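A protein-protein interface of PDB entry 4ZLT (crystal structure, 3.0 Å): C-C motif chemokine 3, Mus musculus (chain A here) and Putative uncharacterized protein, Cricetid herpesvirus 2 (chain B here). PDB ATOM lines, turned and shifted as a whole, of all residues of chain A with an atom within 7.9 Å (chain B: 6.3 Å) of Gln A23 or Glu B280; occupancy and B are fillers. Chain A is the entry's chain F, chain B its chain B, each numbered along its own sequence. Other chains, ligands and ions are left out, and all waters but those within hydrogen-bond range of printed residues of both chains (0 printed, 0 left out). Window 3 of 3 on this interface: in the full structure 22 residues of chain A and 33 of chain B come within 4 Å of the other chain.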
ATOM      1  N   ILE A  20     -13.407 -26.604 -11.333  1.00  0.00           N
ATOM      2  CA  ILE A  20     -14.215 -26.445 -10.123  1.00  0.00           C
ATOM      3  C   ILE A  20     -15.537 -25.801 -10.495  1.00  0.00           C
ATOM      4  O   ILE A  20     -15.652 -25.091 -11.498  1.00  0.00           O
ATOM      5  CB  ILE A  20     -13.501 -25.592  -9.058  1.00  0.00           C
ATOM      6  CG1 ILE A  20     -13.241 -24.183  -9.583  1.00  0.00           C
ATOM      7  CG2 ILE A  20     -12.194 -26.245  -8.653  1.00  0.00           C
ATOM      8  CD1 ILE A  20     -12.470 -23.318  -8.618  1.00  0.00           C
ATOM      9  N   PRO A  21     -16.563 -26.045  -9.683  1.00  0.00           N
ATOM     10  CA  PRO A  21     -17.900 -25.549 -10.030  1.00  0.00           C
ATOM     11  C   PRO A  21     -17.903 -24.044 -10.254  1.00  0.00           C
ATOM     12  O   PRO A  21     -17.208 -23.287  -9.573  1.00  0.00           O
ATOM     13  CB  PRO A  21     -18.749 -25.947  -8.816  1.00  0.00           C
ATOM     14  CG  PRO A  21     -17.765 -26.159  -7.711  1.00  0.00           C
ATOM     15  CD  PRO A  21     -16.541 -26.706  -8.371  1.00  0.00           C
ATOM     16  N   ARG A  22     -18.697 -23.618 -11.238  1.00  0.00           N
ATOM     17  CA  ARG A  22     -18.778 -22.205 -11.586  1.00  0.00           C
ATOM     18  C   ARG A  22     -19.161 -21.345 -10.390  1.00  0.00           C
ATOM     19  O   ARG A  22     -18.713 -20.199 -10.283  1.00  0.00           O
ATOM     20  CB  ARG A  22     -19.781 -22.008 -12.722  1.00  0.00           C
ATOM     21  CG  ARG A  22     -20.138 -20.561 -12.983  1.00  0.00           C
ATOM     22  CD  ARG A  22     -18.925 -19.746 -13.381  1.00  0.00           C
ATOM     23  NE  ARG A  22     -19.288 -18.364 -13.666  1.00  0.00           N
ATOM     24  CZ  ARG A  22     -19.387 -17.415 -12.741  1.00  0.00           C
ATOM     25  NH1 ARG A  22     -19.147 -17.702 -11.468  1.00  0.00           N
ATOM     26  NH2 ARG A  22     -19.723 -16.181 -13.088  1.00  0.00           N
ATOM     27  N   GLN A  23     -19.980 -21.875  -9.485  1.00  0.00           N
ATOM     28  CA  GLN A  23     -20.486 -21.110  -8.353  1.00  0.00           C
ATOM     29  C   GLN A  23     -19.391 -20.689  -7.380  1.00  0.00           C
ATOM     30  O   GLN A  23     -19.674 -20.018  -6.383  1.00  0.00           O
ATOM     31  CB  GLN A  23     -21.544 -21.927  -7.611  1.00  0.00           C
ATOM     32  CG  GLN A  23     -21.067 -23.322  -7.234  1.00  0.00           C
ATOM     33  CD  GLN A  23     -22.124 -24.134  -6.515  1.00  0.00           C
ATOM     34  OE1 GLN A  23     -23.011 -23.586  -5.863  1.00  0.00           O
ATOM     35  NE2 GLN A  23     -22.032 -25.453  -6.630  1.00  0.00           N
ATOM     36  N   PHE A  24     -18.141 -21.067  -7.654  1.00  0.00           N
ATOM     37  CA  PHE A  24     -17.028 -20.719  -6.782  1.00  0.00           C
ATOM     38  C   PHE A  24     -16.137 -19.615  -7.330  1.00  0.00           C
ATOM     39  O   PHE A  24     -15.419 -18.983  -6.550  1.00  0.00           O
ATOM     40  CB  PHE A  24     -16.156 -21.953  -6.501  1.00  0.00           C
ATOM     41  CG  PHE A  24     -16.856 -23.025  -5.715  1.00  0.00           C
ATOM     42  CD1 PHE A  24     -18.118 -22.807  -5.189  1.00  0.00           C
ATOM     43  CD2 PHE A  24     -16.248 -24.248  -5.493  1.00  0.00           C
ATOM     44  CE1 PHE A  24     -18.763 -23.790  -4.467  1.00  0.00           C
ATOM     45  CE2 PHE A  24     -16.885 -25.233  -4.768  1.00  0.00           C
ATOM     46  CZ  PHE A  24     -18.144 -25.004  -4.255  1.00  0.00           C
ATOM     47  N   ILE A  25     -16.167 -19.367  -8.637  1.00  0.00           N
ATOM     48  CA  ILE A  25     -15.315 -18.364  -9.265  1.00  0.00           C
ATOM     49  C   ILE A  25     -16.027 -17.020  -9.226  1.00  0.00           C
ATOM     50  O   ILE A  25     -17.219 -16.929  -9.542  1.00  0.00           O
ATOM     51  CB  ILE A  25     -14.973 -18.763 -10.709  1.00  0.00           C
ATOM     52  CG1 ILE A  25     -14.198 -20.080 -10.726  1.00  0.00           C
ATOM     53  CG2 ILE A  25     -14.175 -17.664 -11.387  1.00  0.00           C
ATOM     54  CD1 ILE A  25     -12.901 -20.027  -9.961  1.00  0.00           C
ATOM     55  N   VAL A  26     -15.298 -15.977  -8.836  1.00  0.00           N
ATOM     56  CA  VAL A  26     -15.877 -14.644  -8.713  1.00  0.00           C
ATOM     57  C   VAL A  26     -15.221 -13.673  -9.690  1.00  0.00           C
ATOM     58  O   VAL A  26     -15.847 -12.699 -10.119  1.00  0.00           O
ATOM     59  CB  VAL A  26     -15.763 -14.135  -7.265  1.00  0.00           C
ATOM     60  CG1 VAL A  26     -16.405 -12.772  -7.130  1.00  0.00           C
ATOM     61  CG2 VAL A  26     -16.415 -15.119  -6.314  1.00  0.00           C
ATOM     62  N   THR A  44     -11.374 -16.665  -6.375  1.00  0.00           N
ATOM     63  CA  THR A  44     -12.504 -17.401  -5.828  1.00  0.00           C
ATOM     64  C   THR A  44     -13.232 -16.576  -4.776  1.00  0.00           C
ATOM     65  O   THR A  44     -12.736 -15.558  -4.287  1.00  0.00           O
ATOM     66  CB  THR A  44     -12.038 -18.727  -5.229  1.00  0.00           C
ATOM     67  OG1 THR A  44     -11.120 -18.469  -4.160  1.00  0.00           O
ATOM     68  CG2 THR A  44     -11.355 -19.573  -6.289  1.00  0.00           C
ATOM     69  N   LYS A  45     -14.434 -17.038  -4.423  1.00  0.00           N
ATOM     70  CA  LYS A  45     -15.205 -16.373  -3.382  1.00  0.00           C
ATOM     71  C   LYS A  45     -14.507 -16.408  -2.032  1.00  0.00           C
ATOM     72  O   LYS A  45     -14.936 -15.703  -1.113  1.00  0.00           O
ATOM     73  CB  LYS A  45     -16.598 -16.994  -3.279  1.00  0.00           C
ATOM     74  CG  LYS A  45     -16.612 -18.466  -2.932  1.00  0.00           C
ATOM     75  CD  LYS A  45     -18.025 -19.023  -3.011  1.00  0.00           C
ATOM     76  CE  LYS A  45     -18.969 -18.279  -2.081  1.00  0.00           C
ATOM     77  NZ  LYS A  45     -20.369 -18.775  -2.206  1.00  0.00           N
ATOM     78  N   TYR A  62     -15.862 -20.349 -18.368  1.00  0.00           N
ATOM     79  CA  TYR A  62     -15.868 -19.527 -17.163  1.00  0.00           C
ATOM     80  C   TYR A  62     -15.502 -18.083 -17.476  1.00  0.00           C
ATOM     81  O   TYR A  62     -16.026 -17.156 -16.854  1.00  0.00           O
ATOM     82  CB  TYR A  62     -14.912 -20.103 -16.121  1.00  0.00           C
ATOM     83  CG  TYR A  62     -15.473 -21.268 -15.341  1.00  0.00           C
ATOM     84  CD1 TYR A  62     -16.609 -21.935 -15.769  1.00  0.00           C
ATOM     85  CD2 TYR A  62     -14.874 -21.687 -14.164  1.00  0.00           C
ATOM     86  CE1 TYR A  62     -17.127 -22.993 -15.051  1.00  0.00           C
ATOM     87  CE2 TYR A  62     -15.382 -22.742 -13.441  1.00  0.00           C
ATOM     88  CZ  TYR A  62     -16.509 -23.393 -13.888  1.00  0.00           C
ATOM     89  OH  TYR A  62     -17.017 -24.449 -13.166  1.00  0.00           O
ATOM     90  N   TYR B 275     -14.461 -26.546   0.939  1.00  0.00           N
ATOM     91  CA  TYR B 275     -15.644 -25.711   0.779  1.00  0.00           C
ATOM     92  C   TYR B 275     -16.808 -26.456   0.138  1.00  0.00           C
ATOM     93  O   TYR B 275     -17.909 -25.901   0.059  1.00  0.00           O
ATOM     94  CB  TYR B 275     -15.295 -24.463  -0.042  1.00  0.00           C
ATOM     95  CG  TYR B 275     -16.461 -23.527  -0.294  1.00  0.00           C
ATOM     96  CD1 TYR B 275     -17.247 -23.066   0.752  1.00  0.00           C
ATOM     97  CD2 TYR B 275     -16.769 -23.098  -1.579  1.00  0.00           C
ATOM     98  CE1 TYR B 275     -18.313 -22.210   0.526  1.00  0.00           C
ATOM     99  CE2 TYR B 275     -17.829 -22.241  -1.815  1.00  0.00           C
ATOM    100  CZ  TYR B 275     -18.598 -21.801  -0.760  1.00  0.00           C
ATOM    101  OH  TYR B 275     -19.656 -20.950  -0.992  1.00  0.00           O
ATOM    102  N   CYS B 278     -19.447 -26.421   2.817  1.00  0.00           N
ATOM    103  CA  CYS B 278     -19.779 -25.189   3.517  1.00  0.00           C
ATOM    104  C   CYS B 278     -21.053 -24.578   2.951  1.00  0.00           C
ATOM    105  O   CYS B 278     -21.279 -24.583   1.738  1.00  0.00           O
ATOM    106  CB  CYS B 278     -18.635 -24.186   3.410  1.00  0.00           C
ATOM    107  SG  CYS B 278     -17.213 -24.616   4.392  1.00  0.00           S
ATOM    108  N   GLU B 279     -21.883 -24.045   3.840  1.00  0.00           N
ATOM    109  CA  GLU B 279     -23.130 -23.428   3.417  1.00  0.00           C
ATOM    110  C   GLU B 279     -22.856 -22.298   2.434  1.00  0.00           C
ATOM    111  O   GLU B 279     -21.937 -21.499   2.625  1.00  0.00           O
ATOM    112  CB  GLU B 279     -23.899 -22.902   4.628  1.00  0.00           C
ATOM    113  CG  GLU B 279     -24.273 -23.972   5.646  1.00  0.00           C
ATOM    114  CD  GLU B 279     -23.099 -24.426   6.498  1.00  0.00           C
ATOM    115  OE1 GLU B 279     -22.089 -23.693   6.572  1.00  0.00           O
ATOM    116  OE2 GLU B 279     -23.186 -25.518   7.093  1.00  0.00           O
ATOM    117  N   GLU B 280     -23.661 -22.241   1.369  1.00  0.00           N
ATOM    118  CA  GLU B 280     -23.513 -21.176   0.382  1.00  0.00           C
ATOM    119  C   GLU B 280     -23.552 -19.807   1.043  1.00  0.00           C
ATOM    120  O   GLU B 280     -22.832 -18.888   0.636  1.00  0.00           O
ATOM    121  CB  GLU B 280     -24.611 -21.286  -0.677  1.00  0.00           C
ATOM    122  CG  GLU B 280     -24.643 -22.613  -1.420  1.00  0.00           C
ATOM    123  CD  GLU B 280     -23.473 -22.785  -2.370  1.00  0.00           C
ATOM    124  OE1 GLU B 280     -22.497 -22.010  -2.268  1.00  0.00           O
ATOM    125  OE2 GLU B 280     -23.532 -23.694  -3.225  1.00  0.00           O
ATOM    126  N   VAL B 281     -24.388 -19.652   2.065  1.00  0.00           N
ATOM    127  CA  VAL B 281     -24.480 -18.423   2.843  1.00  0.00           C
ATOM    128  C   VAL B 281     -24.301 -18.807   4.305  1.00  0.00           C
ATOM    129  O   VAL B 281     -25.170 -19.468   4.888  1.00  0.00           O
ATOM    130  CB  VAL B 281     -25.811 -17.693   2.624  1.00  0.00           C
ATOM    131  CG1 VAL B 281     -26.980 -18.626   2.895  1.00  0.00           C
ATOM    132  CG2 VAL B 281     -25.890 -16.464   3.511  1.00  0.00           C
ATOM    133  N   THR B 282     -23.183 -18.403   4.893  1.00  0.00           N
ATOM    134  CA  THR B 282     -22.883 -18.797   6.262  1.00  0.00           C
ATOM    135  C   THR B 282     -23.989 -18.320   7.195  1.00  0.00           C
ATOM    136  O   THR B 282     -24.315 -17.126   7.202  1.00  0.00           O
ATOM    137  CB  THR B 282     -21.540 -18.229   6.708  1.00  0.00           C
ATOM    138  OG1 THR B 282     -20.512 -18.703   5.833  1.00  0.00           O
ATOM    139  CG2 THR B 282     -21.227 -18.669   8.124  1.00  0.00           C
ATOM    140  N   GLN B 376     -22.641 -10.821  -3.147  1.00  0.00           N
ATOM    141  CA  GLN B 376     -21.819 -11.811  -2.466  1.00  0.00           C
ATOM    142  C   GLN B 376     -20.697 -11.099  -1.727  1.00  0.00           C
ATOM    143  O   GLN B 376     -19.941 -10.332  -2.331  1.00  0.00           O
ATOM    144  CB  GLN B 376     -21.246 -12.835  -3.452  1.00  0.00           C
ATOM    145  CG  GLN B 376     -22.249 -13.876  -3.933  1.00  0.00           C
ATOM    146  CD  GLN B 376     -22.600 -14.895  -2.859  1.00  0.00           C
ATOM    147  OE1 GLN B 376     -21.796 -15.181  -1.972  1.00  0.00           O
ATOM    148  NE2 GLN B 376     -23.806 -15.447  -2.937  1.00  0.00           N
ATOM    149  N   TYR B 395     -19.502 -16.190   4.540  1.00  0.00           N
ATOM    150  CA  TYR B 395     -19.978 -15.847   3.206  1.00  0.00           C
ATOM    151  C   TYR B 395     -21.320 -15.137   3.330  1.00  0.00           C
ATOM    152  O   TYR B 395     -22.287 -15.719   3.829  1.00  0.00           O
ATOM    153  CB  TYR B 395     -20.108 -17.094   2.334  1.00  0.00           C
ATOM    154  CG  TYR B 395     -18.883 -17.973   2.347  1.00  0.00           C
ATOM    155  CD1 TYR B 395     -17.775 -17.662   1.578  1.00  0.00           C
ATOM    156  CD2 TYR B 395     -18.839 -19.118   3.124  1.00  0.00           C
ATOM    157  CE1 TYR B 395     -16.655 -18.463   1.587  1.00  0.00           C
ATOM    158  CE2 TYR B 395     -17.725 -19.926   3.140  1.00  0.00           C
ATOM    159  CZ  TYR B 395     -16.634 -19.596   2.370  1.00  0.00           C
ATOM    160  OH  TYR B 395     -15.518 -20.401   2.383  1.00  0.00           O
ATOM    161  N   LEU B 396     -21.377 -13.891   2.869  1.00  0.00           N
ATOM    162  CA  LEU B 396     -22.570 -13.067   2.994  1.00  0.00           C
ATOM    163  C   LEU B 396     -23.292 -12.947   1.661  1.00  0.00           C
ATOM    164  O   LEU B 396     -22.674 -12.959   0.593  1.00  0.00           O
ATOM    165  CB  LEU B 396     -22.223 -11.668   3.500  1.00  0.00           C
ATOM    166  CG  LEU B 396     -21.520 -11.537   4.847  1.00  0.00           C
ATOM    167  CD1 LEU B 396     -20.057 -11.896   4.710  1.00  0.00           C
ATOM    168  CD2 LEU B 396     -21.684 -10.130   5.387  1.00  0.00           C
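Phe A24 touches Tyr B275. Lys A45 touches Gln B376 (NZ to OE1, 3.9 Å). CE of Lys A45 touches CD1 of Tyr B395, 3.9 Å away.
The side-chain hydroxyl of Tyr B275 sits at hydrogen-bond distance from the side-chain amino group of Lys A45, at 2.6 Å. OE2 of Glu B280 sits close to OE1 of Gln A23 (2.7 Å). The side-chain carboxylate (OE1) of Glu B280 lies within salt-bridge range of the side-chain amino group (NZ) of Lys A45 (3.9 Å).
OH of Tyr B275 is in hydrogen-bond range of OE1 of Glu B280 (3.3 Å). The side-chain hydroxyl (OG1) of Thr B282 is in hydrogen-bond range of the backbone NH (N) of Tyr B395, 3.0 Å away. O of Phe A24 sits at hydrogen-bond distance from N of Lys A45 (3.0 Å).
Of chain B, only Glu B280 (2.7 Å) comes within 4 Å of Gln A23. Of chain A, only Gln A23 (2.7 Å) and Lys A45 (3.8 Å) come within 4 Å of Glu B280. Of the printed residues of chain A, Gln B376 touches Lys A45. Of the printed residues of chain B, Phe A24 touches Tyr B275. Ile A20 touches none of the printed residues of chain B. Cys B278 touches none of the printed residues of chain A. The nearest residue of chain A that does not touch Glu B280 is Phe A24 (4.7 Å). The nearest printed residue of chain B that does not touch Lys A45 is Glu B279 (5.8 Å).
Hydrophobic or aromatic side chains of chain A within 4 Å of the printed part of chain B: Phe A24. Printed residues of chain B that touch a printed residue of chain A: Tyr B275, Glu B280, Gln B376 and Tyr B395. Among the printed residues, 6 pairs touch across the chains. Among the printed residues, Asp or Glu carboxylates within 4 Å of a Lys or Arg side-chain nitrogen of the other chain: Lys A45 with Glu B280 (3.9 Å).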
